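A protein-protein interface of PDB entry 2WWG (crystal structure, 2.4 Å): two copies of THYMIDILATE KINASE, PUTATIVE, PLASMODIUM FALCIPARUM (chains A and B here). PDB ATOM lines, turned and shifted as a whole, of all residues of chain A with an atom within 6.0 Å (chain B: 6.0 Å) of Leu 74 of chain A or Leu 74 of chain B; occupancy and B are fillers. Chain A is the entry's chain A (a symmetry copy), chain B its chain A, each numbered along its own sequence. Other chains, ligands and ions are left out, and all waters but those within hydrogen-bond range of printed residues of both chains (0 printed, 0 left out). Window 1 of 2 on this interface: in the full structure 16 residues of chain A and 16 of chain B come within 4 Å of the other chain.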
ATOM      1  N   ASN A  69      18.427  32.888 -28.352  1.00  0.00           N
ATOM      2  CA  ASN A  69      19.096  31.911 -29.169  1.00  0.00           C
ATOM      3  C   ASN A  69      19.195  30.562 -28.419  1.00  0.00           C
ATOM      4  O   ASN A  69      18.971  29.497 -28.999  1.00  0.00           O
ATOM      5  CB  ASN A  69      20.494  32.398 -29.600  1.00  0.00           C
ATOM      6  CG  ASN A  69      20.465  33.674 -30.478  1.00  0.00           C
ATOM      7  OD1 ASN A  69      21.461  34.418 -30.522  1.00  0.00           O
ATOM      8  ND2 ASN A  69      19.351  33.940 -31.158  1.00  0.00           N
ATOM      9  N   GLU A  70      19.525  30.627 -27.134  1.00  0.00           N
ATOM     10  CA  GLU A  70      19.713  29.457 -26.315  1.00  0.00           C
ATOM     11  C   GLU A  70      18.438  28.643 -26.190  1.00  0.00           C
ATOM     12  O   GLU A  70      18.473  27.427 -26.224  1.00  0.00           O
ATOM     13  CB  GLU A  70      20.182  29.882 -24.926  1.00  0.00           C
ATOM     14  CG  GLU A  70      21.616  30.382 -24.862  1.00  0.00           C
ATOM     15  CD  GLU A  70      21.744  31.859 -25.242  1.00  0.00           C
ATOM     16  OE1 GLU A  70      20.735  32.476 -25.574  1.00  0.00           O
ATOM     17  OE2 GLU A  70      22.865  32.417 -25.250  1.00  0.00           O
ATOM     18  N   THR A  71      17.306  29.303 -26.080  1.00  0.00           N
ATOM     19  CA  THR A  71      16.042  28.626 -25.891  1.00  0.00           C
ATOM     20  C   THR A  71      15.613  27.868 -27.144  1.00  0.00           C
ATOM     21  O   THR A  71      15.180  26.742 -27.070  1.00  0.00           O
ATOM     22  CB  THR A  71      14.935  29.700 -25.540  1.00  0.00           C
ATOM     23  OG1 THR A  71      15.370  30.432 -24.377  1.00  0.00           O
ATOM     24  CG2 THR A  71      13.566  29.049 -25.298  1.00  0.00           C
ATOM     25  N   ILE A  72      15.682  28.516 -28.301  1.00  0.00           N
ATOM     26  CA  ILE A  72      15.294  27.850 -29.518  1.00  0.00           C
ATOM     27  C   ILE A  72      16.242  26.665 -29.804  1.00  0.00           C
ATOM     28  O   ILE A  72      15.772  25.577 -30.065  1.00  0.00           O
ATOM     29  CB  ILE A  72      15.131  28.836 -30.723  1.00  0.00           C
ATOM     30  CG1 ILE A  72      14.398  28.133 -31.851  1.00  0.00           C
ATOM     31  CG2 ILE A  72      16.416  29.338 -31.199  1.00  0.00           C
ATOM     32  CD1 ILE A  72      12.974  27.651 -31.509  1.00  0.00           C
ATOM     33  N   HIS A  73      17.547  26.828 -29.576  1.00  0.00           N
ATOM     34  CA  HIS A  73      18.470  25.683 -29.743  1.00  0.00           C
ATOM     35  C   HIS A  73      18.089  24.492 -28.881  1.00  0.00           C
ATOM     36  O   HIS A  73      18.168  23.349 -29.318  1.00  0.00           O
ATOM     37  CB  HIS A  73      19.943  26.047 -29.520  1.00  0.00           C
ATOM     38  CG  HIS A  73      20.868  24.864 -29.688  1.00  0.00           C
ATOM     39  ND1 HIS A  73      21.039  24.214 -30.898  1.00  0.00           N
ATOM     40  CD2 HIS A  73      21.610  24.181 -28.786  1.00  0.00           C
ATOM     41  CE1 HIS A  73      21.834  23.178 -30.715  1.00  0.00           C
ATOM     42  NE2 HIS A  73      22.216  23.155 -29.451  1.00  0.00           N
ATOM     43  N   LEU A  74      17.640  24.754 -27.664  1.00  0.00           N
ATOM     44  CA  LEU A  74      17.402  23.684 -26.747  1.00  0.00           C
ATOM     45  C   LEU A  74      16.077  23.047 -27.108  1.00  0.00           C
ATOM     46  O   LEU A  74      15.871  21.834 -26.895  1.00  0.00           O
ATOM     47  CB  LEU A  74      17.468  24.191 -25.293  1.00  0.00           C
ATOM     48  CG  LEU A  74      18.847  24.541 -24.697  1.00  0.00           C
ATOM     49  CD1 LEU A  74      18.758  25.229 -23.313  1.00  0.00           C
ATOM     50  CD2 LEU A  74      19.693  23.257 -24.536  1.00  0.00           C
ATOM     51  N   LEU A  75      15.161  23.839 -27.650  1.00  0.00           N
ATOM     52  CA  LEU A  75      13.930  23.265 -28.128  1.00  0.00           C
ATOM     53  C   LEU A  75      14.192  22.329 -29.317  1.00  0.00           C
ATOM     54  O   LEU A  75      13.559  21.304 -29.417  1.00  0.00           O
ATOM     55  CB  LEU A  75      12.976  24.348 -28.548  1.00  0.00           C
ATOM     56  CG  LEU A  75      12.359  25.136 -27.397  1.00  0.00           C
ATOM     57  CD1 LEU A  75      11.160  25.854 -27.880  1.00  0.00           C
ATOM     58  CD2 LEU A  75      12.021  24.215 -26.250  1.00  0.00           C
ATOM     59  N   PHE A  76      15.068  22.709 -30.248  1.00  0.00           N
ATOM     60  CA  PHE A  76      15.386  21.845 -31.375  1.00  0.00           C
ATOM     61  C   PHE A  76      15.968  20.558 -30.913  1.00  0.00           C
ATOM     62  O   PHE A  76      15.588  19.518 -31.432  1.00  0.00           O
ATOM     63  CB  PHE A  76      16.408  22.467 -32.287  1.00  0.00           C
ATOM     64  CG  PHE A  76      15.826  23.324 -33.326  1.00  0.00           C
ATOM     65  CD1 PHE A  76      15.046  22.747 -34.385  1.00  0.00           C
ATOM     66  CD2 PHE A  76      16.046  24.702 -33.287  1.00  0.00           C
ATOM     67  CE1 PHE A  76      14.485  23.562 -35.411  1.00  0.00           C
ATOM     68  CE2 PHE A  76      15.493  25.553 -34.323  1.00  0.00           C
ATOM     69  CZ  PHE A  76      14.720  24.974 -35.419  1.00  0.00           C
ATOM     70  N   SER A  77      16.858  20.626 -29.929  1.00  0.00           N
ATOM     71  CA  SER A  77      17.489  19.453 -29.362  1.00  0.00           C
ATOM     72  C   SER A  77      16.513  18.588 -28.609  1.00  0.00           C
ATOM     73  O   SER A  77      16.519  17.371 -28.757  1.00  0.00           O
ATOM     74  CB  SER A  77      18.603  19.891 -28.423  1.00  0.00           C
ATOM     75  OG  SER A  77      19.289  18.757 -28.003  1.00  0.00           O
ATOM     76  N   ALA A  78      15.626  19.206 -27.815  1.00  0.00           N
ATOM     77  CA  ALA A  78      14.536  18.467 -27.195  1.00  0.00           C
ATOM     78  C   ALA A  78      13.641  17.759 -28.224  1.00  0.00           C
ATOM     79  O   ALA A  78      13.208  16.640 -27.999  1.00  0.00           O
ATOM     80  CB  ALA A  78      13.693  19.387 -26.355  1.00  0.00           C
ATOM     81  N   ASN A  79      13.270  18.447 -29.288  1.00  0.00           N
ATOM     82  CA  ASN A  79      12.484  17.839 -30.379  1.00  0.00           C
ATOM     83  C   ASN A  79      13.264  16.571 -30.925  1.00  0.00           C
ATOM     84  O   ASN A  79      12.701  15.493 -31.071  1.00  0.00           O
ATOM     85  CB  ASN A  79      12.271  18.936 -31.445  1.00  0.00           C
ATOM     86  CG  ASN A  79      11.344  18.534 -32.589  1.00  0.00           C
ATOM     87  OD1 ASN A  79      11.743  18.572 -33.734  1.00  0.00           O
ATOM     88  ND2 ASN A  79      10.110  18.193 -32.285  1.00  0.00           N
ATOM     89  N   TRP A  81      15.315  14.722 -29.200  1.00  0.00           N
ATOM     90  CA  TRP A  81      15.247  13.664 -28.180  1.00  0.00           C
ATOM     91  C   TRP A  81      13.876  12.975 -28.064  1.00  0.00           C
ATOM     92  O   TRP A  81      13.790  11.827 -27.624  1.00  0.00           O
ATOM     93  CB  TRP A  81      15.699  14.207 -26.822  1.00  0.00           C
ATOM     94  CG  TRP A  81      17.188  14.171 -26.649  1.00  0.00           C
ATOM     95  CD1 TRP A  81      18.084  15.236 -26.795  1.00  0.00           C
ATOM     96  CD2 TRP A  81      17.977  13.026 -26.291  1.00  0.00           C
ATOM     97  NE1 TRP A  81      19.370  14.808 -26.551  1.00  0.00           N
ATOM     98  CE2 TRP A  81      19.340  13.451 -26.265  1.00  0.00           C
ATOM     99  CE3 TRP A  81      17.672  11.672 -26.049  1.00  0.00           C
ATOM    100  CZ2 TRP A  81      20.398  12.581 -25.931  1.00  0.00           C
ATOM    101  CZ3 TRP A  81      18.736  10.781 -25.714  1.00  0.00           C
ATOM    102  CH2 TRP A  81      20.091  11.239 -25.690  1.00  0.00           C
ATOM    103  N   TRP A 120      28.877  24.330 -26.895  1.00  0.00           N
ATOM    104  CA  TRP A 120      27.677  24.485 -26.111  1.00  0.00           C
ATOM    105  C   TRP A 120      26.489  23.926 -26.907  1.00  0.00           C
ATOM    106  O   TRP A 120      25.692  23.190 -26.318  1.00  0.00           O
ATOM    107  CB  TRP A 120      27.452  25.947 -25.742  1.00  0.00           C
ATOM    108  CG  TRP A 120      26.288  26.144 -24.860  1.00  0.00           C
ATOM    109  CD1 TRP A 120      26.288  26.181 -23.495  1.00  0.00           C
ATOM    110  CD2 TRP A 120      24.913  26.303 -25.273  1.00  0.00           C
ATOM    111  NE1 TRP A 120      24.994  26.378 -23.032  1.00  0.00           N
ATOM    112  CE2 TRP A 120      24.141  26.457 -24.103  1.00  0.00           C
ATOM    113  CE3 TRP A 120      24.273  26.333 -26.521  1.00  0.00           C
ATOM    114  CZ2 TRP A 120      22.762  26.637 -24.135  1.00  0.00           C
ATOM    115  CZ3 TRP A 120      22.908  26.504 -26.565  1.00  0.00           C
ATOM    116  CH2 TRP A 120      22.159  26.663 -25.368  1.00  0.00           C
ATOM    117  N   PRO A 124      24.026  19.214 -25.773  1.00  0.00           N
ATOM    118  CA  PRO A 124      22.756  18.554 -25.449  1.00  0.00           C
ATOM    119  C   PRO A 124      22.392  17.403 -26.407  1.00  0.00           C
ATOM    120  O   PRO A 124      21.624  16.508 -26.026  1.00  0.00           O
ATOM    121  CB  PRO A 124      21.731  19.680 -25.584  1.00  0.00           C
ATOM    122  CG  PRO A 124      22.414  20.729 -26.365  1.00  0.00           C
ATOM    123  CD  PRO A 124      23.841  20.661 -25.935  1.00  0.00           C
ATOM    124  N   ASP A 125      22.900  17.466 -27.655  1.00  0.00           N
ATOM    125  CA  ASP A 125      22.658  16.408 -28.611  1.00  0.00           C
ATOM    126  C   ASP A 125      23.573  15.210 -28.390  1.00  0.00           C
ATOM    127  O   ASP A 125      23.403  14.140 -28.998  1.00  0.00           O
ATOM    128  CB  ASP A 125      22.788  16.952 -30.026  1.00  0.00           C
ATOM    129  CG  ASP A 125      21.632  17.912 -30.422  1.00  0.00           C
ATOM    130  OD1 ASP A 125      20.425  17.625 -30.153  1.00  0.00           O
ATOM    131  OD2 ASP A 125      21.939  18.941 -31.054  1.00  0.00           O
ATOM    132  N   ASN B  69      13.398  11.368 -20.505  1.00  0.00           N
ATOM    133  CA  ASN B  69      14.079  12.108 -19.476  1.00  0.00           C
ATOM    134  C   ASN B  69      14.841  13.305 -20.089  1.00  0.00           C
ATOM    135  O   ASN B  69      14.824  14.413 -19.548  1.00  0.00           O
ATOM    136  CB  ASN B  69      15.038  11.206 -18.673  1.00  0.00           C
ATOM    137  CG  ASN B  69      14.324  10.060 -17.912  1.00  0.00           C
ATOM    138  OD1 ASN B  69      14.953   9.030 -17.612  1.00  0.00           O
ATOM    139  ND2 ASN B  69      13.036  10.219 -17.611  1.00  0.00           N
ATOM    140  N   GLU B  70      15.498  13.066 -21.220  1.00  0.00           N
ATOM    141  CA  GLU B  70      16.302  14.062 -21.882  1.00  0.00           C
ATOM    142  C   GLU B  70      15.471  15.247 -22.339  1.00  0.00           C
ATOM    143  O   GLU B  70      15.898  16.381 -22.232  1.00  0.00           O
ATOM    144  CB  GLU B  70      16.994  13.432 -23.088  1.00  0.00           C
ATOM    145  CG  GLU B  70      18.129  12.479 -22.746  1.00  0.00           C
ATOM    146  CD  GLU B  70      17.636  11.067 -22.425  1.00  0.00           C
ATOM    147  OE1 GLU B  70      16.430  10.840 -22.442  1.00  0.00           O
ATOM    148  OE2 GLU B  70      18.450  10.168 -22.112  1.00  0.00           O
ATOM    149  N   THR B  71      14.271  14.997 -22.817  1.00  0.00           N
ATOM    150  CA  THR B  71      13.423  16.047 -23.339  1.00  0.00           C
ATOM    151  C   THR B  71      12.919  16.970 -22.232  1.00  0.00           C
ATOM    152  O   THR B  71      12.929  18.170 -22.373  1.00  0.00           O
ATOM    153  CB  THR B  71      12.180  15.387 -24.060  1.00  0.00           C
ATOM    154  OG1 THR B  71      12.672  14.491 -25.076  1.00  0.00           O
ATOM    155  CG2 THR B  71      11.246  16.443 -24.665  1.00  0.00           C
ATOM    156  N   ILE B  72      12.418  16.398 -21.144  1.00  0.00           N
ATOM    157  CA  ILE B  72      11.930  17.218 -20.065  1.00  0.00           C
ATOM    158  C   ILE B  72      13.089  18.032 -19.447  1.00  0.00           C
ATOM    159  O   ILE B  72      12.952  19.226 -19.281  1.00  0.00           O
ATOM    160  CB  ILE B  72      11.096  16.408 -19.018  1.00  0.00           C
ATOM    161  CG1 ILE B  72      10.338  17.373 -18.123  1.00  0.00           C
ATOM    162  CG2 ILE B  72      11.935  15.531 -18.206  1.00  0.00           C
ATOM    163  CD1 ILE B  72       9.328  18.284 -18.849  1.00  0.00           C
ATOM    164  N   HIS B  73      14.268  17.431 -19.283  1.00  0.00           N
ATOM    165  CA  HIS B  73      15.425  18.209 -18.789  1.00  0.00           C
ATOM    166  C   HIS B  73      15.740  19.412 -19.660  1.00  0.00           C
ATOM    167  O   HIS B  73      16.062  20.484 -19.161  1.00  0.00           O
ATOM    168  CB  HIS B  73      16.688  17.364 -18.580  1.00  0.00           C
ATOM    169  CG  HIS B  73      17.860  18.177 -18.081  1.00  0.00           C
ATOM    170  ND1 HIS B  73      17.869  18.795 -16.842  1.00  0.00           N
ATOM    171  CD2 HIS B  73      19.021  18.525 -18.683  1.00  0.00           C
ATOM    172  CE1 HIS B  73      18.980  19.495 -16.726  1.00  0.00           C
ATOM    173  NE2 HIS B  73      19.706  19.323 -17.815  1.00  0.00           N
ATOM    174  N   LEU B  74      15.615  19.251 -20.968  1.00  0.00           N
ATOM    175  CA  LEU B  74      16.033  20.289 -21.856  1.00  0.00           C
ATOM    176  C   LEU B  74      14.954  21.350 -21.875  1.00  0.00           C
ATOM    177  O   LEU B  74      15.237  22.549 -22.075  1.00  0.00           O
ATOM    178  CB  LEU B  74      16.357  19.713 -23.249  1.00  0.00           C
ATOM    179  CG  LEU B  74      17.651  18.893 -23.424  1.00  0.00           C
ATOM    180  CD1 LEU B  74      17.756  18.202 -24.805  1.00  0.00           C
ATOM    181  CD2 LEU B  74      18.884  19.810 -23.257  1.00  0.00           C
ATOM    182  N   LEU B  75      13.709  20.938 -21.673  1.00  0.00           N
ATOM    183  CA  LEU B  75      12.656  21.915 -21.555  1.00  0.00           C
ATOM    184  C   LEU B  75      12.847  22.771 -20.295  1.00  0.00           C
ATOM    185  O   LEU B  75      12.594  23.952 -20.335  1.00  0.00           O
ATOM    186  CB  LEU B  75      11.316  21.236 -21.497  1.00  0.00           C
ATOM    187  CG  LEU B  75      10.845  20.639 -22.820  1.00  0.00           C
ATOM    188  CD1 LEU B  75       9.390  20.390 -22.755  1.00  0.00           C
ATOM    189  CD2 LEU B  75      11.192  21.559 -23.965  1.00  0.00           C
ATOM    190  N   PHE B  76      13.226  22.170 -19.167  1.00  0.00           N
ATOM    191  CA  PHE B  76      13.462  22.936 -17.953  1.00  0.00           C
ATOM    192  C   PHE B  76      14.549  23.930 -18.150  1.00  0.00           C
ATOM    193  O   PHE B  76      14.403  25.062 -17.715  1.00  0.00           O
ATOM    194  CB  PHE B  76      13.896  22.057 -16.810  1.00  0.00           C
ATOM    195  CG  PHE B  76      12.780  21.501 -16.040  1.00  0.00           C
ATOM    196  CD1 PHE B  76      11.959  22.359 -15.233  1.00  0.00           C
ATOM    197  CD2 PHE B  76      12.527  20.127 -16.083  1.00  0.00           C
ATOM    198  CE1 PHE B  76      10.878  21.834 -14.465  1.00  0.00           C
ATOM    199  CE2 PHE B  76      11.439  19.565 -15.306  1.00  0.00           C
ATOM    200  CZ  PHE B  76      10.614  20.427 -14.462  1.00  0.00           C
ATOM    201  N   SER B  77      15.617  23.517 -18.826  1.00  0.00           N
ATOM    202  CA  SER B  77      16.741  24.380 -19.116  1.00  0.00           C
ATOM    203  C   SER B  77      16.383  25.481 -20.080  1.00  0.00           C
ATOM    204  O   SER B  77      16.750  26.632 -19.873  1.00  0.00           O
ATOM    205  CB  SER B  77      17.872  23.547 -19.702  1.00  0.00           C
ATOM    206  OG  SER B  77      18.989  24.362 -19.837  1.00  0.00           O
ATOM    207  N   ALA B  78      15.620  25.153 -21.134  1.00  0.00           N
ATOM    208  CA  ALA B  78      15.078  26.179 -22.011  1.00  0.00           C
ATOM    209  C   ALA B  78      14.207  27.198 -21.260  1.00  0.00           C
ATOM    210  O   ALA B  78      14.260  28.385 -21.545  1.00  0.00           O
ATOM    211  CB  ALA B  78      14.268  25.551 -23.112  1.00  0.00           C
ATOM    212  N   ASN B  79      13.327  26.731 -20.394  1.00  0.00           N
ATOM    213  CA  ASN B  79      12.502  27.623 -19.557  1.00  0.00           C
ATOM    214  C   ASN B  79      13.459  28.585 -18.737  1.00  0.00           C
ATOM    215  O   ASN B  79      13.272  29.795 -18.709  1.00  0.00           O
ATOM    216  CB  ASN B  79      11.627  26.717 -18.662  1.00  0.00           C
ATOM    217  CG  ASN B  79      10.591  27.465 -17.828  1.00  0.00           C
ATOM    218  OD1 ASN B  79      10.593  27.357 -16.620  1.00  0.00           O
ATOM    219  ND2 ASN B  79       9.692  28.183 -18.468  1.00  0.00           N
ATOM    220  N   TRP B  81      16.425  29.550 -19.671  1.00  0.00           N
ATOM    221  CA  TRP B  81      17.022  30.515 -20.608  1.00  0.00           C
ATOM    222  C   TRP B  81      16.061  31.615 -21.092  1.00  0.00           C
ATOM    223  O   TRP B  81      16.498  32.701 -21.477  1.00  0.00           O
ATOM    224  CB  TRP B  81      17.650  29.782 -21.795  1.00  0.00           C
ATOM    225  CG  TRP B  81      19.045  29.309 -21.514  1.00  0.00           C
ATOM    226  CD1 TRP B  81      19.448  28.015 -21.163  1.00  0.00           C
ATOM    227  CD2 TRP B  81      20.240  30.105 -21.559  1.00  0.00           C
ATOM    228  NE1 TRP B  81      20.813  27.977 -20.989  1.00  0.00           N
ATOM    229  CE2 TRP B  81      21.325  29.248 -21.199  1.00  0.00           C
ATOM    230  CE3 TRP B  81      20.492  31.469 -21.810  1.00  0.00           C
ATOM    231  CZ2 TRP B  81      22.661  29.696 -21.156  1.00  0.00           C
ATOM    232  CZ3 TRP B  81      21.841  31.934 -21.764  1.00  0.00           C
ATOM    233  CH2 TRP B  81      22.906  31.049 -21.406  1.00  0.00           C
ATOM    234  N   TRP B 120      26.033  15.859 -18.323  1.00  0.00           N
ATOM    235  CA  TRP B 120      25.142  16.073 -19.437  1.00  0.00           C
ATOM    236  C   TRP B 120      24.029  17.038 -19.003  1.00  0.00           C
ATOM    237  O   TRP B 120      23.738  17.965 -19.764  1.00  0.00           O
ATOM    238  CB  TRP B 120      24.564  14.752 -19.932  1.00  0.00           C
ATOM    239  CG  TRP B 120      23.721  14.909 -21.130  1.00  0.00           C
ATOM    240  CD1 TRP B 120      24.116  14.802 -22.433  1.00  0.00           C
ATOM    241  CD2 TRP B 120      22.315  15.240 -21.156  1.00  0.00           C
ATOM    242  NE1 TRP B 120      23.031  15.024 -23.271  1.00  0.00           N
ATOM    243  CE2 TRP B 120      21.923  15.291 -22.510  1.00  0.00           C
ATOM    244  CE3 TRP B 120      21.359  15.491 -20.159  1.00  0.00           C
ATOM    245  CZ2 TRP B 120      20.620  15.584 -22.901  1.00  0.00           C
ATOM    246  CZ3 TRP B 120      20.069  15.789 -20.535  1.00  0.00           C
ATOM    247  CH2 TRP B 120      19.704  15.825 -21.907  1.00  0.00           C
ATOM    248  N   PRO B 124      23.739  22.234 -20.571  1.00  0.00           N
ATOM    249  CA  PRO B 124      22.919  23.263 -21.225  1.00  0.00           C
ATOM    250  C   PRO B 124      22.693  24.517 -20.360  1.00  0.00           C
ATOM    251  O   PRO B 124      22.418  25.596 -20.905  1.00  0.00           O
ATOM    252  CB  PRO B 124      21.587  22.552 -21.461  1.00  0.00           C
ATOM    253  CG  PRO B 124      21.614  21.378 -20.568  1.00  0.00           C
ATOM    254  CD  PRO B 124      23.041  20.943 -20.549  1.00  0.00           C
ATOM    255  N   ASP B 125      22.752  24.355 -19.023  1.00  0.00           N
ATOM    256  CA  ASP B 125      22.604  25.481 -18.127  1.00  0.00           C
ATOM    257  C   ASP B 125      23.888  26.293 -18.003  1.00  0.00           C
ATOM    258  O   ASP B 125      23.912  27.388 -17.418  1.00  0.00           O
ATOM    259  CB  ASP B 125      22.116  25.000 -16.770  1.00  0.00           C
ATOM    260  CG  ASP B 125      20.644  24.503 -16.788  1.00  0.00           C
ATOM    261  OD1 ASP B 125      19.741  25.162 -17.389  1.00  0.00           O
ATOM    262  OD2 ASP B 125      20.386  23.466 -16.148  1.00  0.00           O
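O of Pro 124 of chain A sits close to NE1 of Trp 120 of chain B, 3.4 Å away.
The indole nitrogen (NE1) of Trp 120 of chain A lies close to the backbone carbonyl oxygen (O) of Pro 124 of chain B, 3.4 Å away.
The side-chain hydroxyl (OG) of Ser 77 of chain B sits at hydrogen-bond distance from the side-chain carboxylate (OD1) of Asp 125 of chain B, at 2.7 Å.
O of Pro 124 of chain B lies within hydrogen-bond range of NE1 of Trp 81 of chain B (2.9 Å).
The side-chain hydroxyl (OG) of Ser 77 of chain A lies within hydrogen-bond range of the side-chain carboxylate (OD1) of Asp 125 of chain A (2.7 Å).
The indole nitrogen (NE1) of Trp 81 of chain A is in hydrogen-bond range of the backbone carbonyl oxygen (O) of Pro 124 of chain A, at 2.9 Å.
CB of Glu 70 of chain A touches CD2 of Trp 81 of chain B (3.4 Å).
OG1 of Thr 71 of chain A touches CB of Trp 81 of chain B (3.5 Å).
CD2 of Leu 74 of chain A touches CD2 of Leu 74 of chain B, 3.8 Å away.
Leu 74 of chain A touches Ser 77 of chain B (CD1 to OG, 3.6 Å).
Leu 75 of chain A touches Leu 75 of chain B.
OG of Ser 77 of chain A touches CD1 of Leu 74 of chain B, at 3.6 Å.
Glu 70 of chain B touches Trp 81 of chain A.
Trp 81 of chain A touches Leu 74 of chain B.
Trp 120 of chain B touches Trp 81 of chain A.
Leu 74 of chain B touches Pro 124 of chain A.
Printed residues of chain A within 4 Å of Trp 120 of chain B: Trp 81 and Pro 124.
Of the printed residues of chain A, Ser 77 of chain B touches Leu 74 (3.6 Å).
Of the printed residues of chain B, Trp 81 of chain A touches Glu 70 (3.4 Å), Thr 71 (3.5 Å), Leu 74 (3.6 Å) and Trp 120 (3.9 Å).
Printed residues of chain B within 4 Å of Ala 78 of chain A: Thr 71 and Leu 74.
The nearest residue of chain A that does not touch Leu 74 of chain B is Leu 75 of chain A (5.5 Å).
Printed residues of chain A that touch a printed residue of chain B: Glu 70, Thr 71, Leu 74, Leu 75, Ser 77, Ala 78, Trp 81, Trp 120 and Pro 124.
Along chain A the printed residues that touch a printed residue of chain B span positions 70 to 124.
Hydrophobic or aromatic side chains of chain B within 4 Å of the printed part of chain A: Leu 74, Leu 75, Trp 81, Trp 120 and Pro 124.
Among the printed residues, no Asp or Glu carboxylate lies within 4 Å of a Lys or Arg side-chain nitrogen of the other chain.
Thr 71 of chain A touches Ala 78 of chain B, and with the chains exchanged Ala 78 of chain A touches Thr 71 of chain B.
Leu 74 of chain B touches its own counterpart, Leu 74 of chain A.
Leu 74 of chain A touches Ser 77 of chain B, and with the chains exchanged Ser 77 of chain A touches Leu 74 of chain B.
Leu 75 of chain B touches its own counterpart, Leu 75 of chain A.
15 positions are printed for both chains.
Of the 20 pairs that touch across the chains among the printed residues, 20 have their exchanged pair printed and touching as well.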
